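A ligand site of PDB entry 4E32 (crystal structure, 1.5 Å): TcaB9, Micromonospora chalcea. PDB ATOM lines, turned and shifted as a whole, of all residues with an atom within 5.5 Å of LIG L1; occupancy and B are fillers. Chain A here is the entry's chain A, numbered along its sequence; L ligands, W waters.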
ATOM      1  N   ASP A  35     -10.982 -18.603  25.476  1.00  0.00           N
ATOM      2  CA  ASP A  35     -11.841 -18.307  24.321  1.00  0.00           C
ATOM      3  C   ASP A  35     -13.317 -18.289  24.694  1.00  0.00           C
ATOM      4  O   ASP A  35     -14.137 -18.413  23.783  1.00  0.00           O
ATOM      5  CB  ASP A  35     -11.513 -19.289  23.179  1.00  0.00           C
ATOM      6  CG  ASP A  35     -10.464 -18.765  22.240  1.00  0.00           C
ATOM      7  OD1 ASP A  35     -10.606 -17.602  21.809  1.00  0.00           O
ATOM      8  OD2 ASP A  35      -9.517 -19.524  21.942  1.00  0.00           O
ATOM      9  N   TYR A  78     -16.924 -22.479  19.722  1.00  0.00           N
ATOM     10  CA  TYR A  78     -15.558 -21.966  19.711  1.00  0.00           C
ATOM     11  C   TYR A  78     -15.451 -20.812  18.735  1.00  0.00           C
ATOM     12  O   TYR A  78     -15.854 -20.901  17.583  1.00  0.00           O
ATOM     13  CB  TYR A  78     -14.638 -23.062  19.206  1.00  0.00           C
ATOM     14  CG  TYR A  78     -13.159 -22.751  19.258  1.00  0.00           C
ATOM     15  CD1 TYR A  78     -12.419 -22.589  18.082  1.00  0.00           C
ATOM     16  CD2 TYR A  78     -12.505 -22.705  20.491  1.00  0.00           C
ATOM     17  CE1 TYR A  78     -11.046 -22.352  18.113  1.00  0.00           C
ATOM     18  CE2 TYR A  78     -11.111 -22.454  20.537  1.00  0.00           C
ATOM     19  CZ  TYR A  78     -10.408 -22.305  19.341  1.00  0.00           C
ATOM     20  OH  TYR A  78      -9.045 -22.089  19.366  1.00  0.00           O
ATOM     21  N   TYR A  80     -12.751 -18.860  17.458  1.00  0.00           N
ATOM     22  CA  TYR A  80     -11.649 -18.286  16.659  1.00  0.00           C
ATOM     23  C   TYR A  80     -11.818 -18.661  15.199  1.00  0.00           C
ATOM     24  O   TYR A  80     -12.022 -19.843  14.878  1.00  0.00           O
ATOM     25  CB  TYR A  80     -10.325 -18.923  17.081  1.00  0.00           C
ATOM     26  CG  TYR A  80      -9.173 -18.393  16.257  1.00  0.00           C
ATOM     27  CD1 TYR A  80      -8.768 -17.068  16.391  1.00  0.00           C
ATOM     28  CD2 TYR A  80      -8.444 -19.283  15.453  1.00  0.00           C
ATOM     29  CE1 TYR A  80      -7.684 -16.597  15.671  1.00  0.00           C
ATOM     30  CE2 TYR A  80      -7.363 -18.798  14.723  1.00  0.00           C
ATOM     31  CZ  TYR A  80      -7.015 -17.471  14.863  1.00  0.00           C
ATOM     32  OH  TYR A  80      -5.912 -17.007  14.180  1.00  0.00           O
ATOM     33  N   GLY A  84      -9.715 -14.911   9.453  1.00  0.00           N
ATOM     34  CA  GLY A  84      -9.770 -13.480   9.713  1.00  0.00           C
ATOM     35  C   GLY A  84      -8.466 -12.743   9.509  1.00  0.00           C
ATOM     36  O   GLY A  84      -8.424 -11.529   9.732  1.00  0.00           O
ATOM     37  N   SER A  85      -7.395 -13.383   9.068  1.00  0.00           N
ATOM     38  CA  SER A  85      -6.112 -12.710   8.830  1.00  0.00           C
ATOM     39  C   SER A  85      -5.700 -13.044   7.403  1.00  0.00           C
ATOM     40  O   SER A  85      -5.597 -14.205   6.990  1.00  0.00           O
ATOM     41  CB  SER A  85      -5.049 -13.282   9.748  1.00  0.00           C
ATOM     42  OG  SER A  85      -3.738 -13.019   9.297  1.00  0.00           O
ATOM     43  N   SER A  86      -5.424 -11.968   6.680  1.00  0.00           N
ATOM     44  CA  SER A  86      -4.918 -12.070   5.307  1.00  0.00           C
ATOM     45  C   SER A  86      -3.520 -12.686   5.258  1.00  0.00           C
ATOM     46  O   SER A  86      -3.226 -13.518   4.375  1.00  0.00           O
ATOM     47  CB  SER A  86      -4.945 -10.705   4.640  1.00  0.00           C
ATOM     48  OG  SER A  86      -3.956  -9.790   5.156  1.00  0.00           O
ATOM     49  N   ASN A 179      -1.000 -25.008  14.769  1.00  0.00           N
ATOM     50  CA  ASN A 179      -1.547 -24.362  15.992  1.00  0.00           C
ATOM     51  C   ASN A 179      -2.593 -25.298  16.591  1.00  0.00           C
ATOM     52  O   ASN A 179      -3.615 -24.835  17.102  1.00  0.00           O
ATOM     53  CB  ASN A 179      -2.186 -23.015  15.625  1.00  0.00           C
ATOM     54  CG  ASN A 179      -1.144 -22.168  14.883  1.00  0.00           C
ATOM     55  OD1 ASN A 179      -0.096 -21.925  15.525  1.00  0.00           O
ATOM     56  ND2 ASN A 179      -1.349 -21.758  13.623  1.00  0.00           N
ATOM     57  N   HIS A 183      -1.989 -28.001  21.445  1.00  0.00           N
ATOM     58  CA  HIS A 183      -3.192 -27.814  22.255  1.00  0.00           C
ATOM     59  C   HIS A 183      -3.613 -29.141  22.879  1.00  0.00           C
ATOM     60  O   HIS A 183      -4.541 -29.149  23.702  1.00  0.00           O
ATOM     61  CB  HIS A 183      -4.373 -27.428  21.343  1.00  0.00           C
ATOM     62  CG  HIS A 183      -4.238 -26.068  20.721  1.00  0.00           C
ATOM     63  ND1 HIS A 183      -3.042 -25.553  20.270  1.00  0.00           N
ATOM     64  CD2 HIS A 183      -5.179 -25.124  20.471  1.00  0.00           C
ATOM     65  CE1 HIS A 183      -3.251 -24.323  19.828  1.00  0.00           C
ATOM     66  NE2 HIS A 183      -4.540 -24.052  19.900  1.00  0.00           N
ATOM     67  N   TYR A 224      -1.499 -20.230  27.784  1.00  0.00           N
ATOM     68  CA  TYR A 224      -2.890 -20.095  28.202  1.00  0.00           C
ATOM     69  C   TYR A 224      -3.474 -21.500  27.977  1.00  0.00           C
ATOM     70  O   TYR A 224      -2.762 -22.424  27.513  1.00  0.00           O
ATOM     71  CB  TYR A 224      -3.609 -19.009  27.413  1.00  0.00           C
ATOM     72  CG  TYR A 224      -3.699 -19.141  25.907  1.00  0.00           C
ATOM     73  CD1 TYR A 224      -4.831 -19.713  25.305  1.00  0.00           C
ATOM     74  CD2 TYR A 224      -2.702 -18.634  25.067  1.00  0.00           C
ATOM     75  CE1 TYR A 224      -4.949 -19.805  23.921  1.00  0.00           C
ATOM     76  CE2 TYR A 224      -2.813 -18.734  23.681  1.00  0.00           C
ATOM     77  CZ  TYR A 224      -3.941 -19.326  23.120  1.00  0.00           C
ATOM     78  OH  TYR A 224      -4.098 -19.444  21.758  1.00  0.00           O
ATOM     79  N   GLU A 226      -5.326 -23.321  26.062  1.00  0.00           N
ATOM     80  CA  GLU A 226      -5.234 -24.070  24.789  1.00  0.00           C
ATOM     81  C   GLU A 226      -3.821 -24.426  24.357  1.00  0.00           C
ATOM     82  O   GLU A 226      -3.632 -25.248  23.443  1.00  0.00           O
ATOM     83  CB  GLU A 226      -5.913 -23.278  23.637  1.00  0.00           C
ATOM     84  CG  GLU A 226      -7.418 -23.226  23.934  1.00  0.00           C
ATOM     85  CD  GLU A 226      -8.148 -22.351  22.922  1.00  0.00           C
ATOM     86  OE1 GLU A 226      -7.727 -22.261  21.728  1.00  0.00           O
ATOM     87  OE2 GLU A 226      -9.163 -21.734  23.335  1.00  0.00           O
ATOM     88  N   HIS A 227      -2.831 -23.833  25.023  1.00  0.00           N
ATOM     89  CA  HIS A 227      -1.438 -24.109  24.637  1.00  0.00           C
ATOM     90  C   HIS A 227      -0.773 -24.952  25.721  1.00  0.00           C
ATOM     91  O   HIS A 227      -0.093 -24.413  26.595  1.00  0.00           O
ATOM     92  CB  HIS A 227      -0.637 -22.828  24.494  1.00  0.00           C
ATOM     93  CG  HIS A 227      -0.926 -22.118  23.205  1.00  0.00           C
ATOM     94  ND1 HIS A 227      -0.299 -20.963  22.803  1.00  0.00           N
ATOM     95  CD2 HIS A 227      -1.815 -22.404  22.212  1.00  0.00           C
ATOM     96  CE1 HIS A 227      -0.782 -20.540  21.648  1.00  0.00           C
ATOM     97  NE2 HIS A 227      -1.705 -21.405  21.269  1.00  0.00           N
ATOM     98  N   HIS A 256       2.377 -15.953  14.173  1.00  0.00           N
ATOM     99  CA  HIS A 256       2.008 -16.181  15.561  1.00  0.00           C
ATOM    100  C   HIS A 256       3.126 -15.974  16.590  1.00  0.00           C
ATOM    101  O   HIS A 256       3.198 -16.703  17.580  1.00  0.00           O
ATOM    102  CB  HIS A 256       1.390 -17.563  15.660  1.00  0.00           C
ATOM    103  CG  HIS A 256       0.017 -17.615  15.062  1.00  0.00           C
ATOM    104  ND1 HIS A 256      -1.019 -16.835  15.501  1.00  0.00           N
ATOM    105  CD2 HIS A 256      -0.472 -18.336  14.017  1.00  0.00           C
ATOM    106  CE1 HIS A 256      -2.100 -17.086  14.775  1.00  0.00           C
ATOM    107  NE2 HIS A 256      -1.779 -17.977  13.843  1.00  0.00           N
ATOM    108  N   TYR A 325      -6.528  -3.740  21.204  1.00  0.00           N
ATOM    109  CA  TYR A 325      -6.766  -4.111  19.808  1.00  0.00           C
ATOM    110  C   TYR A 325      -6.463  -5.600  19.619  1.00  0.00           C
ATOM    111  O   TYR A 325      -5.327  -6.009  19.772  1.00  0.00           O
ATOM    112  CB  TYR A 325      -5.965  -3.195  18.865  1.00  0.00           C
ATOM    113  CG  TYR A 325      -6.575  -3.162  17.472  1.00  0.00           C
ATOM    114  CD1 TYR A 325      -6.638  -4.339  16.711  1.00  0.00           C
ATOM    115  CD2 TYR A 325      -7.062  -1.966  16.946  1.00  0.00           C
ATOM    116  CE1 TYR A 325      -7.222  -4.283  15.424  1.00  0.00           C
ATOM    117  CE2 TYR A 325      -7.611  -1.911  15.680  1.00  0.00           C
ATOM    118  CZ  TYR A 325      -7.683  -3.081  14.911  1.00  0.00           C
ATOM    119  OH  TYR A 325      -8.251  -3.004  13.651  1.00  0.00           O
ATOM    120  N   GLY A 326      -7.530  -6.370  19.387  1.00  0.00           N
ATOM    121  CA  GLY A 326      -7.504  -7.801  19.083  1.00  0.00           C
ATOM    122  C   GLY A 326      -7.926  -8.525  20.368  1.00  0.00           C
ATOM    123  O   GLY A 326      -7.224  -8.543  21.378  1.00  0.00           O
ATOM    124  N   ALA A 327      -9.086  -9.196  20.329  1.00  0.00           N
ATOM    125  CA  ALA A 327      -9.558  -9.949  21.504  1.00  0.00           C
ATOM    126  C   ALA A 327      -8.976 -11.363  21.346  1.00  0.00           C
ATOM    127  O   ALA A 327      -9.702 -12.357  21.201  1.00  0.00           O
ATOM    128  CB  ALA A 327     -11.143  -9.992  21.524  1.00  0.00           C
ATOM    129  N   THR A 328      -7.644 -11.443  21.363  1.00  0.00           N
ATOM    130  CA  THR A 328      -6.899 -12.712  21.310  1.00  0.00           C
ATOM    131  C   THR A 328      -7.203 -13.606  22.499  1.00  0.00           C
ATOM    132  O   THR A 328      -7.493 -13.109  23.594  1.00  0.00           O
ATOM    133  CB  THR A 328      -5.362 -12.455  21.292  1.00  0.00           C
ATOM    134  OG1 THR A 328      -5.052 -11.744  22.506  1.00  0.00           O
ATOM    135  CG2 THR A 328      -4.966 -11.565  20.065  1.00  0.00           C
ATOM    136  N   ALA A 329      -7.192 -14.922  22.272  1.00  0.00           N
ATOM    137  CA  ALA A 329      -7.107 -15.883  23.365  1.00  0.00           C
ATOM    138  C   ALA A 329      -5.910 -15.554  24.295  1.00  0.00           C
ATOM    139  O   ALA A 329      -6.045 -15.561  25.516  1.00  0.00           O
ATOM    140  CB  ALA A 329      -6.986 -17.282  22.781  1.00  0.00           C
ATOM    141  N   LYS A 330      -4.761 -15.223  23.714  1.00  0.00           N
ATOM    142  CA  LYS A 330      -3.559 -14.779  24.422  1.00  0.00           C
ATOM    143  C   LYS A 330      -3.805 -13.704  25.476  1.00  0.00           C
ATOM    144  O   LYS A 330      -3.200 -13.744  26.558  1.00  0.00           O
ATOM    145  CB  LYS A 330      -2.529 -14.221  23.436  1.00  0.00           C
ATOM    146  CG  LYS A 330      -1.988 -15.320  22.482  1.00  0.00           C
ATOM    147  CD  LYS A 330      -0.790 -14.756  21.685  1.00  0.00           C
ATOM    148  CE  LYS A 330      -1.049 -13.616  20.673  1.00  0.00           C
ATOM    149  NZ  LYS A 330      -1.927 -14.145  19.607  1.00  0.00           N
ATOM    150  N   TYR A 349     -11.085  -3.945  20.535  1.00  0.00           N
ATOM    151  CA  TYR A 349     -11.609  -3.893  19.156  1.00  0.00           C
ATOM    152  C   TYR A 349     -11.237  -5.185  18.433  1.00  0.00           C
ATOM    153  O   TYR A 349     -10.113  -5.645  18.528  1.00  0.00           O
ATOM    154  CB  TYR A 349     -11.181  -2.611  18.416  1.00  0.00           C
ATOM    155  CG  TYR A 349     -11.756  -1.411  19.118  1.00  0.00           C
ATOM    156  CD1 TYR A 349     -13.108  -1.101  18.927  1.00  0.00           C
ATOM    157  CD2 TYR A 349     -11.007  -0.661  20.043  1.00  0.00           C
ATOM    158  CE1 TYR A 349     -13.692  -0.042  19.623  1.00  0.00           C
ATOM    159  CE2 TYR A 349     -11.591   0.384  20.739  1.00  0.00           C
ATOM    160  CZ  TYR A 349     -12.924   0.685  20.490  1.00  0.00           C
ATOM    161  OH  TYR A 349     -13.521   1.723  21.169  1.00  0.00           O
ATOM    162  N   ASP A 350     -12.199  -5.836  17.770  1.00  0.00           N
ATOM    163  CA  ASP A 350     -11.947  -7.121  17.135  1.00  0.00           C
ATOM    164  C   ASP A 350     -12.862  -7.390  15.931  1.00  0.00           C
ATOM    165  O   ASP A 350     -14.018  -6.975  16.004  1.00  0.00           O
ATOM    166  CB  ASP A 350     -12.255  -8.231  18.150  1.00  0.00           C
ATOM    167  CG  ASP A 350     -11.677  -9.553  17.720  1.00  0.00           C
ATOM    168  OD1 ASP A 350     -10.505  -9.853  18.049  1.00  0.00           O
ATOM    169  OD2 ASP A 350     -12.463 -10.322  17.121  1.00  0.00           O
ATOM    170  N   THR A 351     -12.354  -8.065  14.898  1.00  0.00           N
ATOM    171  CA  THR A 351     -13.171  -8.281  13.716  1.00  0.00           C
ATOM    172  C   THR A 351     -14.065  -9.511  13.761  1.00  0.00           C
ATOM    173  O   THR A 351     -14.738  -9.742  12.765  1.00  0.00           O
ATOM    174  CB  THR A 351     -12.260  -8.487  12.504  1.00  0.00           C
ATOM    175  OG1 THR A 351     -11.304  -9.500  12.865  1.00  0.00           O
ATOM    176  CG2 THR A 351     -11.568  -7.147  12.237  1.00  0.00           C
ATOM    177  N   THR A 352     -14.039 -10.279  14.849  1.00  0.00           N
ATOM    178  CA  THR A 352     -14.768 -11.530  14.906  1.00  0.00           C
ATOM    179  C   THR A 352     -16.177 -11.306  15.444  1.00  0.00           C
ATOM    180  O   THR A 352     -16.403 -10.958  16.604  1.00  0.00           O
ATOM    181  CB  THR A 352     -14.068 -12.554  15.867  1.00  0.00           C
ATOM    182  OG1 THR A 352     -12.648 -12.508  15.689  1.00  0.00           O
ATOM    183  CG2 THR A 352     -14.620 -13.967  15.675  1.00  0.00           C
ATOM    184  N   LYS A 355     -17.238 -12.632  18.924  1.00  0.00           N
ATOM    185  CA  LYS A 355     -16.602 -12.013  20.083  1.00  0.00           C
ATOM    186  C   LYS A 355     -17.153 -10.619  20.368  1.00  0.00           C
ATOM    187  O   LYS A 355     -16.973 -10.055  21.445  1.00  0.00           O
ATOM    188  CB  LYS A 355     -15.083 -11.866  19.852  1.00  0.00           C
ATOM    189  CG  LYS A 355     -14.398 -13.228  19.683  1.00  0.00           C
ATOM    190  CD  LYS A 355     -12.870 -13.094  19.534  1.00  0.00           C
ATOM    191  CE  LYS A 355     -12.179 -14.449  19.362  1.00  0.00           C
ATOM    192  NZ  LYS A 355     -10.682 -14.170  19.283  1.00  0.00           N
ATOM    193  N   ALA A 370     -14.076  -3.949  15.148  1.00  0.00           N
ATOM    194  CA  ALA A 370     -12.950  -3.075  14.798  1.00  0.00           C
ATOM    195  C   ALA A 370     -13.417  -1.880  13.974  1.00  0.00           C
ATOM    196  O   ALA A 370     -12.765  -0.852  13.942  1.00  0.00           O
ATOM    197  CB  ALA A 370     -11.891  -3.843  14.018  1.00  0.00           C
ATOM    198  N   ALA A 385      -3.138  -8.192  19.671  1.00  0.00           N
ATOM    199  CA  ALA A 385      -2.805  -8.957  18.441  1.00  0.00           C
ATOM    200  C   ALA A 385      -1.459  -8.543  17.842  1.00  0.00           C
ATOM    201  O   ALA A 385      -1.350  -8.215  16.656  1.00  0.00           O
ATOM    202  CB  ALA A 385      -4.001  -8.891  17.454  1.00  0.00           C
ATOM    203  N   ASN A 387       1.124 -10.260  17.208  1.00  0.00           N
ATOM    204  CA  ASN A 387       1.582 -11.097  16.109  1.00  0.00           C
ATOM    205  C   ASN A 387       1.030 -10.719  14.735  1.00  0.00           C
ATOM    206  O   ASN A 387       1.522 -11.251  13.726  1.00  0.00           O
ATOM    207  CB  ASN A 387       1.191 -12.539  16.432  1.00  0.00           C
ATOM    208  CG  ASN A 387      -0.286 -12.713  16.807  1.00  0.00           C
ATOM    209  OD1 ASN A 387      -0.773 -12.111  17.772  1.00  0.00           O
ATOM    210  ND2 ASN A 387      -1.001 -13.559  16.062  1.00  0.00           N
ATOM    211  N   HIS A 388      -0.006  -9.893  14.725  1.00  0.00           N
ATOM    212  CA  HIS A 388      -0.623  -9.345  13.525  1.00  0.00           C
ATOM    213  C   HIS A 388      -0.281  -7.876  13.352  1.00  0.00           C
ATOM    214  O   HIS A 388      -1.040  -7.212  12.643  1.00  0.00           O
ATOM    215  CB  HIS A 388      -2.145  -9.509  13.652  1.00  0.00           C
ATOM    216  CG  HIS A 388      -2.611 -10.928  13.622  1.00  0.00           C
ATOM    217  ND1 HIS A 388      -2.412 -11.720  12.517  1.00  0.00           N
ATOM    218  CD2 HIS A 388      -3.252 -11.709  14.535  1.00  0.00           C
ATOM    219  CE1 HIS A 388      -2.959 -12.918  12.727  1.00  0.00           C
ATOM    220  NE2 HIS A 388      -3.472 -12.932  13.948  1.00  0.00           N
ATOM    221  N   GLU A 391      -0.179  -6.398   9.636  1.00  0.00           N
ATOM    222  CA  GLU A 391      -1.495  -6.418   9.000  1.00  0.00           C
ATOM    223  C   GLU A 391      -2.436  -5.382   9.616  1.00  0.00           C
ATOM    224  O   GLU A 391      -3.154  -4.670   8.915  1.00  0.00           O
ATOM    225  CB  GLU A 391      -2.113  -7.813   9.151  1.00  0.00           C
ATOM    226  CG  GLU A 391      -3.462  -7.924   8.494  1.00  0.00           C
ATOM    227  CD  GLU A 391      -3.929  -9.365   8.443  1.00  0.00           C
ATOM    228  OE1 GLU A 391      -5.127  -9.572   8.202  1.00  0.00           O
ATOM    229  OE2 GLU A 391      -3.125 -10.305   8.630  1.00  0.00           O
ATOM    230  N   ILE A 392      -2.482  -5.363  10.935  1.00  0.00           N
ATOM    231  CA  ILE A 392      -3.374  -4.426  11.632  1.00  0.00           C
ATOM    232  C   ILE A 392      -2.959  -2.969  11.385  1.00  0.00           C
ATOM    233  O   ILE A 392      -3.754  -2.068  11.060  1.00  0.00           O
ATOM    234  CB  ILE A 392      -3.504  -4.746  13.138  1.00  0.00           C
ATOM    235  CG1 ILE A 392      -4.373  -6.003  13.321  1.00  0.00           C
ATOM    236  CG2 ILE A 392      -4.153  -3.529  13.841  1.00  0.00           C
ATOM    237  CD1 ILE A 392      -4.286  -6.667  14.692  1.00  0.00           C
ATOM    238  N   LYS A 395      -3.904  -1.466   8.163  1.00  0.00           N
ATOM    239  CA  LYS A 395      -5.319  -1.115   8.074  1.00  0.00           C
ATOM    240  C   LYS A 395      -5.712   0.082   8.940  1.00  0.00           C
ATOM    241  O   LYS A 395      -6.768   0.670   8.729  1.00  0.00           O
ATOM    242  CB  LYS A 395      -6.146  -2.295   8.578  1.00  0.00           C
ATOM    243  CG  LYS A 395      -6.241  -3.386   7.523  1.00  0.00           C
ATOM    244  CD  LYS A 395      -7.394  -4.317   7.840  1.00  0.00           C
ATOM    245  CE  LYS A 395      -6.913  -5.295   8.877  1.00  0.00           C
ATOM    246  NZ  LYS A 395      -8.044  -6.205   9.188  1.00  0.00           N
HETATM  247  O1  LIG L   1      -3.321 -20.916  18.920  1.00  0.00           O
HETATM  248  C1  LIG L   1      -4.373 -20.373  18.583  1.00  0.00           C
HETATM  249  C2  LIG L   1      -4.342 -19.361  17.475  1.00  0.00           C
HETATM  250  C3  LIG L   1      -4.066 -19.915  16.072  1.00  0.00           C
HETATM  251  O2  LIG L   1      -5.584 -18.722  17.278  1.00  0.00           O
HETATM  252  C4  LIG L   1      -5.729 -20.717  19.142  1.00  0.00           C
HETATM  253  N1  LIG L   1      -5.542 -21.517  20.328  1.00  0.00           N
HETATM  254  C5  LIG L   1      -6.747 -19.584  19.269  1.00  0.00           C
HETATM  255  C6  LIG L   1      -6.262 -18.362  18.481  1.00  0.00           C
HETATM  256  O3  LIG L   1      -5.376 -17.633  19.322  1.00  0.00           O
HETATM  257  P1  LIG L   1      -5.384 -16.021  19.242  1.00  0.00           P
HETATM  258  O4  LIG L   1      -6.811 -15.576  19.542  1.00  0.00           O
HETATM  259  O5  LIG L   1      -4.235 -15.508  20.080  1.00  0.00           O
HETATM  260  O6  LIG L   1      -5.086 -15.759  17.687  1.00  0.00           O
HETATM  261  P2  LIG L   1      -4.800 -14.418  16.811  1.00  0.00           P
HETATM  262  O7  LIG L   1      -4.751 -14.921  15.382  1.00  0.00           O
HETATM  263  O8  LIG L   1      -3.582 -13.732  17.313  1.00  0.00           O
HETATM  264  O9  LIG L   1      -6.135 -13.594  17.110  1.00  0.00           O
HETATM  265  C7  LIG L   1      -6.260 -12.323  16.474  1.00  0.00           C
HETATM  266  C8  LIG L   1      -7.541 -11.700  17.010  1.00  0.00           C
HETATM  267  O10 LIG L   1      -7.468 -10.355  16.554  1.00  0.00           O
HETATM  268  C9  LIG L   1      -8.768 -12.347  16.375  1.00  0.00           C
HETATM  269  O11 LIG L   1      -9.814 -12.296  17.359  1.00  0.00           O
HETATM  270  C10 LIG L   1      -9.055 -11.393  15.249  1.00  0.00           C
HETATM  271  C11 LIG L   1      -8.536 -10.030  15.681  1.00  0.00           C
HETATM  272  N2  LIG L   1      -7.980  -9.351  14.502  1.00  0.00           N
HETATM  273  C12 LIG L   1      -8.479  -8.150  14.179  1.00  0.00           C
HETATM  274  O12 LIG L   1      -9.334  -7.603  14.890  1.00  0.00           O
HETATM  275  N3  LIG L   1      -7.989  -7.451  13.124  1.00  0.00           N
HETATM  276  C13 LIG L   1      -7.046  -9.965  13.747  1.00  0.00           C
HETATM  277  C14 LIG L   1      -6.538  -9.354  12.615  1.00  0.00           C
HETATM  278  C15 LIG L   1      -5.499 -10.010  11.746  1.00  0.00           C
HETATM  279  C16 LIG L   1      -7.099  -8.016  12.288  1.00  0.00           C
HETATM  280  O13 LIG L   1      -6.686  -7.362  11.299  1.00  0.00           O
HETATM  281  N1  LG2 L   2      -5.295 -24.709  12.218  1.00  0.00           N
HETATM  282  C1  LG2 L   2      -5.989 -23.416  12.464  1.00  0.00           C
HETATM  283  C2  LG2 L   2      -6.823 -23.373  13.738  1.00  0.00           C
HETATM  284  C3  LG2 L   2      -5.984 -23.433  15.011  1.00  0.00           C
HETATM  285  S1  LG2 L   2      -6.946 -23.197  16.468  1.00  0.00           S
HETATM  286  C4  LG2 L   2      -4.954 -22.332  12.420  1.00  0.00           C
HETATM  287  O1  LG2 L   2      -3.749 -22.605  12.436  1.00  0.00           O
HETATM  288  O2  LG2 L   2      -5.356 -21.163  12.402  1.00  0.00           O
HETATM  289  C5  LG2 L   2      -6.917 -24.824  17.159  1.00  0.00           C
HETATM  290  C6  LG2 L   2      -7.973 -25.739  16.517  1.00  0.00           C
HETATM  291  O3  LG2 L   2      -7.813 -27.094  16.965  1.00  0.00           O
HETATM  292  C7  LG2 L   2      -9.445 -25.405  16.832  1.00  0.00           C
HETATM  293  O4  LG2 L   2     -10.242 -25.054  15.679  1.00  0.00           O
HETATM  294  C8  LG2 L   2      -9.927 -26.605  17.650  1.00  0.00           C
HETATM  295  O5  LG2 L   2     -11.314 -26.885  17.581  1.00  0.00           O
HETATM  296  C9  LG2 L   2      -9.118 -27.701  16.970  1.00  0.00           C
HETATM  297  N2  LG2 L   2      -8.871 -28.893  17.829  1.00  0.00           N
HETATM  298  C10 LG2 L   2      -8.662 -29.068  19.137  1.00  0.00           C
HETATM  299  N3  LG2 L   2      -8.389 -30.336  19.529  1.00  0.00           N
HETATM  300  C11 LG2 L   2      -8.380 -31.045  18.344  1.00  0.00           C
HETATM  301  C12 LG2 L   2      -8.136 -32.458  17.974  1.00  0.00           C
HETATM  302  N4  LG2 L   2      -7.878 -33.423  18.880  1.00  0.00           N
HETATM  303  N5  LG2 L   2      -8.293 -32.710  16.656  1.00  0.00           N
HETATM  304  C13 LG2 L   2      -8.540 -31.781  15.717  1.00  0.00           C
HETATM  305  N6  LG2 L   2      -8.756 -30.486  15.954  1.00  0.00           N
HETATM  306  C14 LG2 L   2      -8.644 -30.077  17.242  1.00  0.00           C
HETATM  307  O   HOH W   1      -0.590 -20.640  18.103  1.00  0.00           O
HETATM  308  O   HOH W   2      -2.456 -17.839  20.261  1.00  0.00           O
HETATM  309  O   HOH W   3      -9.680  -9.315  10.544  1.00  0.00           O
HETATM  310  O   HOH W   4      -9.663 -14.091  13.303  1.00  0.00           O
HETATM  311  O   HOH W   5      -9.305 -16.502  19.627  1.00  0.00           O
HETATM  312  O   HOH W   6      -8.990  -4.993  12.143  1.00  0.00           O
HETATM  313  O   HOH W   7      -6.946 -13.305  13.048  1.00  0.00           O
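An oxygen (O1) of LG2 L2 lies within hydrogen-bond range of the side-chain amide nitrogen of Asn 179, at 2.8 Å. O11 of LIG L1 is in hydrogen-bond range of OD1 of Asp 350 (2.6 Å). NZ of Lys 330 is in salt-bridge range of O5 of LIG L1 (2.7 Å). The side-chain amide nitrogen (ND2) of Asn 387 lies within hydrogen-bond range of an oxygen (O8) of LIG L1 (2.9 Å). O11 of LIG L1 sits at hydrogen-bond distance from OG1 of Thr 352 (3.3 Å). N of Thr 351 lies within hydrogen-bond range of O12 of LIG L1 (3.1 Å). NZ of Lys 355 sits at hydrogen-bond distance from O11 of LIG L1, 2.8 Å away. A ring nitrogen (NE2) of His 183 is in hydrogen-bond range of a nitrogen (N1) of LIG L1, 2.8 Å away. N1 of LIG L1 lies within salt-bridge range of OE1 of Glu 226 (2.7 Å). The side-chain hydroxyl of Tyr 80 sits at hydrogen-bond distance from an oxygen (O7) of LIG L1. An oxygen (O7) of LIG L1 sits at hydrogen-bond distance from a ring nitrogen (NE2) of His 388. The side-chain hydroxyl (OG1) of Thr 351 lies close to an oxygen (O12) of LIG L1. N1 of LIG L1 lies within hydrogen-bond range of OH of Tyr 224 (2.9 Å). NE2 of His 227 is in hydrogen-bond range of O1 of LIG L1, 2.9 Å away. An oxygen (O4) of LIG L1 is in hydrogen-bond range of the backbone NH (N) of Ala 329, 2.8 Å away. NZ of Lys 395 lies within hydrogen-bond range of O13 of LIG L1 (2.8 Å). A sulfur (S1) of LG2 L2 sits close to the side-chain hydroxyl of Tyr 78 (3.7 Å).
O of Asn 179 sits close to NE2 of His 183 (3.0 Å). The backbone NH of Gly 326 sits at hydrogen-bond distance from the backbone carbonyl oxygen of Tyr 349 (2.8 Å). The side-chain amino group (NZ) of Lys 355 sits at hydrogen-bond distance from the backbone carbonyl oxygen (O) of Ala 327, 2.8 Å away. The side-chain amino group (NZ) of Lys 330 sits at hydrogen-bond distance from the side-chain amide oxygen (OD1) of Asn 387 (3.0 Å). OE2 of Glu 226 lies close to OD2 of Asp 35. The side-chain carboxylate (OD1) of Asp 350 lies within hydrogen-bond range of the backbone NH (N) of Ala 327, 2.8 Å away. A ring nitrogen (NE2) of His 227 is in hydrogen-bond range of the side-chain hydroxyl of Tyr 224 (3.1 Å). O of Asp 350 is in hydrogen-bond range of N of Ala 370, 3.1 Å away.
Residues that only touch LIG L1: Asp 35, Tyr 78, Gly 84, Ser 85, Asn 179, His 256, Tyr 325, Gly 326, Ala 327, Thr 328, Ala 385, Glu 391 and Ile 392. Of the 30 residues printed, 27 come within 4 Å of LIG L1. The nearest printed residue that does not touch LIG L1 is Tyr 349 (4.2 Å).
Water W5 lies within hydrogen-bond range of O4 of LIG L1 (2.7 Å), NZ of Lys 355 (2.7 Å) and OD1 of Asp 35 (2.8 Å). Water W6 lies within hydrogen-bond range of OH of Tyr 325 (2.6 Å), N3 of LIG L1 (2.8 Å) and NZ of Lys 395 (3.3 Å). Water W1 lies within hydrogen-bond range of O1 of LIG L1 (2.9 Å), OD1 of Asn 179 (2.9 Å) and NE2 of His 227 (3.4 Å). Water W2 lies within hydrogen-bond range of OH of Tyr 224 (2.7 Å) and O5 of LIG L1 (2.9 Å). Water W3 lies within hydrogen-bond range of O of Gly 84 (2.7 Å) and OG1 of Thr 351 (2.8 Å).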
